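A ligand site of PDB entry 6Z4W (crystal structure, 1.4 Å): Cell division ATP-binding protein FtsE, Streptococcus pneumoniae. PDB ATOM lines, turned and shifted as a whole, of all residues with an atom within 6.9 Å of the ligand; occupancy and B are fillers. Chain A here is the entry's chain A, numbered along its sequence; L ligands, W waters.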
ATOM      1  N   LYS A  11       5.198   2.194  -3.594  1.00  0.00           N
ATOM      2  CA  LYS A  11       5.351   3.464  -4.290  1.00  0.00           C
ATOM      3  C   LYS A  11       4.183   3.627  -5.242  1.00  0.00           C
ATOM      4  O   LYS A  11       3.969   2.793  -6.124  1.00  0.00           O
ATOM      5  CB  LYS A  11       6.685   3.526  -5.055  1.00  0.00           C
ATOM      6  CG  LYS A  11       6.780   4.712  -6.028  1.00  0.00           C
ATOM      7  CD  LYS A  11       6.670   6.032  -5.309  1.00  0.00           C
ATOM      8  CE  LYS A  11       6.633   7.202  -6.303  1.00  0.00           C
ATOM      9  NZ  LYS A  11       6.752   8.485  -5.586  1.00  0.00           N
ATOM     10  N   TYR A  13       2.540   6.489  -7.838  1.00  0.00           N
ATOM     11  CA  TYR A  13       2.724   7.769  -8.517  1.00  0.00           C
ATOM     12  C   TYR A  13       1.455   8.611  -8.385  1.00  0.00           C
ATOM     13  O   TYR A  13       0.376   8.111  -8.035  1.00  0.00           O
ATOM     14  CB  TYR A  13       3.110   7.554  -9.975  1.00  0.00           C
ATOM     15  CG  TYR A  13       4.516   7.007 -10.151  1.00  0.00           C
ATOM     16  CD1 TYR A  13       5.622   7.837 -10.008  1.00  0.00           C
ATOM     17  CD2 TYR A  13       4.738   5.672 -10.465  1.00  0.00           C
ATOM     18  CE1 TYR A  13       6.910   7.344 -10.168  1.00  0.00           C
ATOM     19  CE2 TYR A  13       6.026   5.169 -10.624  1.00  0.00           C
ATOM     20  CZ  TYR A  13       7.102   6.010 -10.480  1.00  0.00           C
ATOM     21  OH  TYR A  13       8.402   5.537 -10.631  1.00  0.00           O
ATOM     22  N   ASP A  14       1.592   9.902  -8.651  1.00  0.00           N
ATOM     23  CA  ASP A  14       0.504  10.832  -8.371  1.00  0.00           C
ATOM     24  C   ASP A  14      -0.732  10.609  -9.241  1.00  0.00           C
ATOM     25  O   ASP A  14      -1.810  11.080  -8.871  1.00  0.00           O
ATOM     26  CB  ASP A  14       0.952  12.285  -8.527  1.00  0.00           C
ATOM     27  CG  ASP A  14       1.819  12.746  -7.402  1.00  0.00           C
ATOM     28  OD1 ASP A  14       1.865  12.068  -6.338  1.00  0.00           O
ATOM     29  OD2 ASP A  14       2.454  13.803  -7.569  1.00  0.00           O
ATOM     30  N   ASN A  15      -0.594   9.928 -10.375  1.00  0.00           N
ATOM     31  CA  ASN A  15      -1.770   9.605 -11.176  1.00  0.00           C
ATOM     32  C   ASN A  15      -2.465   8.345 -10.710  1.00  0.00           C
ATOM     33  O   ASN A  15      -3.351   7.836 -11.413  1.00  0.00           O
ATOM     34  CB  ASN A  15      -1.412   9.509 -12.666  1.00  0.00           C
ATOM     35  CG  ASN A  15      -0.617   8.267 -12.993  1.00  0.00           C
ATOM     36  OD1 ASN A  15      -0.264   7.486 -12.114  1.00  0.00           O
ATOM     37  ND2 ASN A  15      -0.351   8.079 -14.276  1.00  0.00           N
ATOM     38  N   GLY A  16      -2.069   7.810  -9.548  1.00  0.00           N
ATOM     39  CA  GLY A  16      -2.716   6.652  -8.978  1.00  0.00           C
ATOM     40  C   GLY A  16      -2.095   5.314  -9.313  1.00  0.00           C
ATOM     41  O   GLY A  16      -2.614   4.290  -8.862  1.00  0.00           O
ATOM     42  N   THR A  17      -1.026   5.284 -10.092  1.00  0.00           N
ATOM     43  CA  THR A  17      -0.414   4.006 -10.449  1.00  0.00           C
ATOM     44  C   THR A  17       0.464   3.526  -9.304  1.00  0.00           C
ATOM     45  O   THR A  17       1.418   4.196  -8.920  1.00  0.00           O
ATOM     46  CB  THR A  17       0.435   4.172 -11.721  1.00  0.00           C
ATOM     47  OG1 THR A  17      -0.390   4.622 -12.797  1.00  0.00           O
ATOM     48  CG2 THR A  17       1.075   2.843 -12.078  1.00  0.00           C
ATOM     49  N   THR A  18       0.137   2.348  -8.750  1.00  0.00           N
ATOM     50  CA  THR A  18       0.956   1.747  -7.700  1.00  0.00           C
ATOM     51  C   THR A  18       2.036   0.898  -8.362  1.00  0.00           C
ATOM     52  O   THR A  18       1.798  -0.234  -8.756  1.00  0.00           O
ATOM     53  CB  THR A  18       0.120   0.924  -6.736  1.00  0.00           C
ATOM     54  OG1 THR A  18      -0.872   1.749  -6.108  1.00  0.00           O
ATOM     55  CG2 THR A  18       1.031   0.340  -5.661  1.00  0.00           C
ATOM     56  N   ALA A  19       3.241   1.460  -8.450  1.00  0.00           N
ATOM     57  CA  ALA A  19       4.323   0.850  -9.217  1.00  0.00           C
ATOM     58  C   ALA A  19       5.053  -0.215  -8.422  1.00  0.00           C
ATOM     59  O   ALA A  19       5.522  -1.213  -8.988  1.00  0.00           O
ATOM     60  CB  ALA A  19       5.304   1.920  -9.674  1.00  0.00           C
ATOM     61  N   LEU A  20       5.221   0.000  -7.114  1.00  0.00           N
ATOM     62  CA  LEU A  20       5.720  -1.004  -6.188  1.00  0.00           C
ATOM     63  C   LEU A  20       4.613  -1.258  -5.191  1.00  0.00           C
ATOM     64  O   LEU A  20       4.147  -0.328  -4.524  1.00  0.00           O
ATOM     65  CB  LEU A  20       6.985  -0.516  -5.486  1.00  0.00           C
ATOM     66  CG  LEU A  20       8.171  -0.142  -6.390  1.00  0.00           C
ATOM     67  CD1 LEU A  20       9.294   0.443  -5.592  1.00  0.00           C
ATOM     68  CD2 LEU A  20       8.652  -1.375  -7.151  1.00  0.00           C
ATOM     69  N   GLY A  37      11.137  -9.003 -15.728  1.00  0.00           N
ATOM     70  CA  GLY A  37       9.699  -8.869 -15.713  1.00  0.00           C
ATOM     71  C   GLY A  37       9.212  -8.031 -16.876  1.00  0.00           C
ATOM     72  O   GLY A  37       9.980  -7.329 -17.534  1.00  0.00           O
ATOM     73  N   PRO A  38       7.913  -8.078 -17.155  1.00  0.00           N
ATOM     74  CA  PRO A  38       7.399  -7.400 -18.343  1.00  0.00           C
ATOM     75  C   PRO A  38       7.504  -5.879 -18.211  1.00  0.00           C
ATOM     76  O   PRO A  38       7.610  -5.326 -17.127  1.00  0.00           O
ATOM     77  CB  PRO A  38       5.947  -7.858 -18.435  1.00  0.00           C
ATOM     78  CG  PRO A  38       5.597  -8.296 -17.054  1.00  0.00           C
ATOM     79  CD  PRO A  38       6.874  -8.851 -16.461  1.00  0.00           C
ATOM     80  N   SER A  39       7.473  -5.214 -19.366  1.00  0.00           N
ATOM     81  CA  SER A  39       7.398  -3.761 -19.383  1.00  0.00           C
ATOM     82  C   SER A  39       6.227  -3.305 -18.507  1.00  0.00           C
ATOM     83  O   SER A  39       5.144  -3.903 -18.536  1.00  0.00           O
ATOM     84  CB  SER A  39       7.216  -3.278 -20.816  1.00  0.00           C
ATOM     85  OG  SER A  39       7.226  -1.859 -20.887  1.00  0.00           O
ATOM     86  N   GLY A  40       6.473  -2.273 -17.701  1.00  0.00           N
ATOM     87  CA  GLY A  40       5.456  -1.741 -16.796  1.00  0.00           C
ATOM     88  C   GLY A  40       5.377  -2.428 -15.445  1.00  0.00           C
ATOM     89  O   GLY A  40       4.553  -2.024 -14.617  1.00  0.00           O
ATOM     90  N   ALA A  41       6.220  -3.439 -15.199  1.00  0.00           N
ATOM     91  CA  ALA A  41       6.152  -4.219 -13.966  1.00  0.00           C
ATOM     92  C   ALA A  41       6.603  -3.424 -12.745  1.00  0.00           C
ATOM     93  O   ALA A  41       6.134  -3.684 -11.633  1.00  0.00           O
ATOM     94  CB  ALA A  41       7.006  -5.479 -14.106  1.00  0.00           C
ATOM     95  N   GLY A  42       7.535  -2.475 -12.927  1.00  0.00           N
ATOM     96  CA  GLY A  42       8.079  -1.696 -11.841  1.00  0.00           C
ATOM     97  C   GLY A  42       9.576  -1.808 -11.690  1.00  0.00           C
ATOM     98  O   GLY A  42      10.125  -1.401 -10.667  1.00  0.00           O
ATOM     99  N   LYS A  43      10.266  -2.353 -12.708  1.00  0.00           N
ATOM    100  CA  LYS A  43      11.708  -2.564 -12.591  1.00  0.00           C
ATOM    101  C   LYS A  43      12.450  -1.232 -12.440  1.00  0.00           C
ATOM    102  O   LYS A  43      13.313  -1.097 -11.558  1.00  0.00           O
ATOM    103  CB  LYS A  43      12.231  -3.338 -13.795  1.00  0.00           C
ATOM    104  CG  LYS A  43      11.547  -4.683 -13.990  1.00  0.00           C
ATOM    105  CD  LYS A  43      12.099  -5.467 -15.175  1.00  0.00           C
ATOM    106  CE  LYS A  43      11.920  -4.732 -16.513  1.00  0.00           C
ATOM    107  NZ  LYS A  43      10.491  -4.528 -16.931  1.00  0.00           N
ATOM    108  N   SER A  44      12.144  -0.261 -13.285  1.00  0.00           N
ATOM    109  CA  SER A  44      12.822   1.032 -13.170  1.00  0.00           C
ATOM    110  C   SER A  44      12.474   1.723 -11.863  1.00  0.00           C
ATOM    111  O   SER A  44      13.329   2.342 -11.222  1.00  0.00           O
ATOM    112  CB  SER A  44      12.456   1.926 -14.351  1.00  0.00           C
ATOM    113  OG  SER A  44      13.038   1.441 -15.554  1.00  0.00           O
ATOM    114  N   THR A  45      11.211   1.631 -11.432  1.00  0.00           N
ATOM    115  CA  THR A  45      10.858   2.251 -10.164  1.00  0.00           C
ATOM    116  C   THR A  45      11.642   1.614  -9.011  1.00  0.00           C
ATOM    117  O   THR A  45      12.132   2.310  -8.121  1.00  0.00           O
ATOM    118  CB  THR A  45       9.344   2.152  -9.939  1.00  0.00           C
ATOM    119  OG1 THR A  45       8.675   2.798 -11.018  1.00  0.00           O
ATOM    120  CG2 THR A  45       8.955   2.834  -8.640  1.00  0.00           C
ATOM    121  N   PHE A  46      11.768   0.288  -9.049  1.00  0.00           N
ATOM    122  CA  PHE A  46      12.561  -0.433  -8.055  1.00  0.00           C
ATOM    123  C   PHE A  46      14.008   0.063  -8.065  1.00  0.00           C
ATOM    124  O   PHE A  46      14.538   0.451  -7.020  1.00  0.00           O
ATOM    125  CB  PHE A  46      12.476  -1.929  -8.379  1.00  0.00           C
ATOM    126  CG  PHE A  46      13.327  -2.806  -7.505  1.00  0.00           C
ATOM    127  CD1 PHE A  46      14.606  -3.184  -7.918  1.00  0.00           C
ATOM    128  CD2 PHE A  46      12.877  -3.274  -6.289  1.00  0.00           C
ATOM    129  CE1 PHE A  46      15.383  -4.020  -7.131  1.00  0.00           C
ATOM    130  CE2 PHE A  46      13.653  -4.111  -5.522  1.00  0.00           C
ATOM    131  CZ  PHE A  46      14.913  -4.458  -5.934  1.00  0.00           C
ATOM    132  N   ARG A  48      15.295   2.819  -9.226  1.00  0.00           N
ATOM    133  CA  ARG A  48      15.458   4.233  -8.894  1.00  0.00           C
ATOM    134  C   ARG A  48      15.195   4.515  -7.423  1.00  0.00           C
ATOM    135  O   ARG A  48      15.716   5.503  -6.882  1.00  0.00           O
ATOM    136  CB  ARG A  48      14.613   5.088  -9.828  1.00  0.00           C
ATOM    137  CG  ARG A  48      14.998   4.902 -11.308  1.00  0.00           C
ATOM    138  CD  ARG A  48      14.290   5.913 -12.202  1.00  0.00           C
ATOM    139  NE  ARG A  48      12.955   6.235 -11.706  1.00  0.00           N
ATOM    140  CZ  ARG A  48      11.842   6.182 -12.435  1.00  0.00           C
ATOM    141  NH1 ARG A  48      11.902   5.811 -13.713  1.00  0.00           N
ATOM    142  NH2 ARG A  48      10.678   6.490 -11.888  1.00  0.00           N
ATOM    143  N   ASP A 164      21.029  -0.735 -15.663  1.00  0.00           N
ATOM    144  CA  ASP A 164      19.710  -0.809 -16.290  1.00  0.00           C
ATOM    145  C   ASP A 164      19.900  -1.189 -17.755  1.00  0.00           C
ATOM    146  O   ASP A 164      20.283  -0.349 -18.585  1.00  0.00           O
ATOM    147  CB  ASP A 164      18.988   0.527 -16.159  1.00  0.00           C
ATOM    148  CG  ASP A 164      17.530   0.441 -16.579  1.00  0.00           C
ATOM    149  OD1 ASP A 164      17.064  -0.655 -16.961  1.00  0.00           O
ATOM    150  OD2 ASP A 164      16.863   1.492 -16.545  1.00  0.00           O
ATOM    151  N   HIS A 197      16.363  -7.972 -20.122  1.00  0.00           N
ATOM    152  CA  HIS A 197      15.434  -8.792 -20.895  1.00  0.00           C
ATOM    153  C   HIS A 197      16.169  -9.864 -21.703  1.00  0.00           C
ATOM    154  O   HIS A 197      15.570 -10.487 -22.599  1.00  0.00           O
ATOM    155  CB  HIS A 197      14.598  -7.928 -21.850  1.00  0.00           C
ATOM    156  CG  HIS A 197      13.518  -7.129 -21.177  1.00  0.00           C
ATOM    157  ND1 HIS A 197      12.214  -7.549 -21.137  1.00  0.00           N
ATOM    158  CD2 HIS A 197      13.549  -5.935 -20.553  1.00  0.00           C
ATOM    159  CE1 HIS A 197      11.485  -6.652 -20.495  1.00  0.00           C
ATOM    160  NE2 HIS A 197      12.268  -5.656 -20.128  1.00  0.00           N
ATOM    161  N   ILE A 212       9.553  -9.363 -11.256  1.00  0.00           N
ATOM    162  CA  ILE A 212       8.546  -8.421 -10.781  1.00  0.00           C
ATOM    163  C   ILE A 212       7.410  -8.380 -11.792  1.00  0.00           C
ATOM    164  O   ILE A 212       7.648  -8.315 -12.998  1.00  0.00           O
ATOM    165  CB  ILE A 212       9.151  -7.014 -10.594  1.00  0.00           C
ATOM    166  CG1 ILE A 212      10.333  -7.067  -9.635  1.00  0.00           C
ATOM    167  CG2 ILE A 212       8.107  -6.030 -10.097  1.00  0.00           C
ATOM    168  CD1 ILE A 212      11.073  -5.756  -9.503  1.00  0.00           C
ATOM    169  N   ASN A 214       3.431  -6.374 -12.059  1.00  0.00           N
ATOM    170  CA  ASN A 214       2.407  -5.519 -11.480  1.00  0.00           C
ATOM    171  C   ASN A 214       2.778  -5.097 -10.057  1.00  0.00           C
ATOM    172  O   ASN A 214       1.964  -5.161  -9.120  1.00  0.00           O
ATOM    173  CB  ASN A 214       1.031  -6.199 -11.531  1.00  0.00           C
ATOM    174  CG  ASN A 214      -0.106  -5.238 -11.239  1.00  0.00           C
ATOM    175  OD1 ASN A 214      -0.002  -4.036 -11.501  1.00  0.00           O
ATOM    176  ND2 ASN A 214      -1.205  -5.762 -10.697  1.00  0.00           N
ATOM    177  N   GLY A 215       4.042  -4.701  -9.874  1.00  0.00           N
ATOM    178  CA  GLY A 215       4.488  -4.165  -8.608  1.00  0.00           C
ATOM    179  C   GLY A 215       4.805  -5.171  -7.531  1.00  0.00           C
ATOM    180  O   GLY A 215       5.050  -4.761  -6.392  1.00  0.00           O
HETATM  181  P1  LIG L   1       9.331  -1.117 -15.909  1.00  0.00           P
HETATM  182  O1  LIG L   1      10.679  -0.491 -15.625  1.00  0.00           O
HETATM  183  O2  LIG L   1       9.223  -2.534 -15.422  1.00  0.00           O
HETATM  184  O3  LIG L   1       8.927  -0.969 -17.362  1.00  0.00           O
HETATM  185  P2  LIG L   1       8.270   1.229 -14.479  1.00  0.00           P
HETATM  186  O4  LIG L   1       8.905   2.128 -15.474  1.00  0.00           O
HETATM  187  O5  LIG L   1       8.834   1.194 -13.096  1.00  0.00           O
HETATM  188  O6  LIG L   1       8.262  -0.265 -15.057  1.00  0.00           O
HETATM  189  O7  LIG L   1       6.700   1.539 -14.400  1.00  0.00           O
HETATM  190  C1  LIG L   1       5.902   0.866 -13.390  1.00  0.00           C
HETATM  191  C2  LIG L   1       4.496   1.428 -13.416  1.00  0.00           C
HETATM  192  O8  LIG L   1       4.524   2.799 -12.936  1.00  0.00           O
HETATM  193  C3  LIG L   1       3.823   1.507 -14.793  1.00  0.00           C
HETATM  194  O9  LIG L   1       2.412   1.372 -14.683  1.00  0.00           O
HETATM  195  C4  LIG L   1       4.222   2.905 -15.266  1.00  0.00           C
HETATM  196  O10 LIG L   1       3.335   3.420 -16.230  1.00  0.00           O
HETATM  197  C5  LIG L   1       4.167   3.687 -13.957  1.00  0.00           C
HETATM  198  N1  LIG L   1       5.076   4.831 -13.921  1.00  0.00           N
HETATM  199  C6  LIG L   1       6.426   4.805 -14.144  1.00  0.00           C
HETATM  200  N2  LIG L   1       6.990   5.982 -14.040  1.00  0.00           N
HETATM  201  C7  LIG L   1       5.951   6.841 -13.731  1.00  0.00           C
HETATM  202  C8  LIG L   1       5.898   8.229 -13.488  1.00  0.00           C
HETATM  203  N3  LIG L   1       6.972   9.016 -13.533  1.00  0.00           N
HETATM  204  N4  LIG L   1       4.698   8.772 -13.203  1.00  0.00           N
HETATM  205  C9  LIG L   1       3.622   7.965 -13.168  1.00  0.00           C
HETATM  206  N5  LIG L   1       3.550   6.651 -13.366  1.00  0.00           N
HETATM  207  C10 LIG L   1       4.761   6.138 -13.651  1.00  0.00           C
HETATM  208  O   HOH W   1       9.650   4.683 -15.229  1.00  0.00           O
HETATM  209  O   HOH W   2       9.938   8.058 -14.285  1.00  0.00           O
HETATM  210  O   HOH W   3      10.961   2.115 -17.669  1.00  0.00           O
HETATM  211  O   HOH W   4       1.603  -0.674 -12.873  1.00  0.00           O
HETATM  212  O   HOH W   5       1.519   6.293 -15.531  1.00  0.00           O
HETATM  213  O   HOH W   6      12.459   0.033 -17.476  1.00  0.00           O
HETATM  214  O   HOH W   7       4.422  11.212 -11.928  1.00  0.00           O
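O of Ala 41 lies within hydrogen-bond range of N of Gly 215, 2.9 Å away.
NZ of Lys 43 sits at hydrogen-bond distance from O of Gly 37 (2.9 Å).
OG1 of Thr 45 sits at hydrogen-bond distance from OH of Tyr 13.
O of Lys 11 is in hydrogen-bond range of N of Ala 19, at 2.8 Å.
OD1 of Asn 15 is in hydrogen-bond range of OG1 of Thr 17 (2.9 Å).
OH of Tyr 13 is in hydrogen-bond range of NH2 of Arg 48 (2.8 Å).
The side-chain amino group of Lys 43 lies within hydrogen-bond range of the backbone carbonyl oxygen of Pro 38 (3.0 Å).
Water W6 bridges the side-chain hydroxyl (OG) of Ser 44 (2.5 Å) and an oxygen (O1) of the ligand (2.6 Å).
Water W1 lies within hydrogen-bond range of O4 of the ligand and NH1 of Arg 48.
Water W5 lies within hydrogen-bond range of the side-chain amide nitrogen of Asn 15 (2.9 Å) and a nitrogen (N5) of the ligand (3.0 Å).
Water W3 lies within hydrogen-bond range of an oxygen (O4) of the ligand (3.0 Å) and the side-chain hydroxyl (OG) of Ser 44 (3.0 Å).
Water W2 lies within hydrogen-bond range of NH2 of Arg 48 and N3 of the ligand.
Tyr 13 touches the ligand.
Thr 17 touches the ligand.
Ala 19 touches the ligand (CB to O8, 3.5 Å).
Pro 38 touches the ligand (O to O2, 3.6 Å).
C of Ser 39 touches O3 of the ligand (3.7 Å).
Within 4 Å of the ligand: Tyr 13, Thr 17, Ala 19, Pro 38, Ser 39, Gly 40, Ala 41, Gly 42, Lys 43, Ser 44 and Thr 45.
An oxygen (O3) of the ligand is in hydrogen-bond range of the backbone NH (N) of Gly 40 (2.8 Å).
The backbone NH of Ala 41 sits at hydrogen-bond distance from an oxygen (O2) of the ligand (3.1 Å).
An oxygen (O5) of the ligand lies within hydrogen-bond range of the side-chain hydroxyl (OG1) of Thr 45 (2.6 Å).
N of Gly 42 lies within hydrogen-bond range of O2 of the ligand.
The side-chain amino group (NZ) of Lys 43 lies within salt-bridge range of an oxygen (O2) of the ligand, 2.8 Å away.
The side-chain hydroxyl of Ser 44 sits at hydrogen-bond distance from an oxygen (O1) of the ligand (3.1 Å).
The backbone NH (N) of Ser 44 is in hydrogen-bond range of an oxygen (O1) of the ligand.
An oxygen (O5) of the ligand lies within hydrogen-bond range of the backbone NH of Thr 45, 2.9 Å away.
O2 of the ligand lies within hydrogen-bond range of N of Lys 43, 2.9 Å away.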
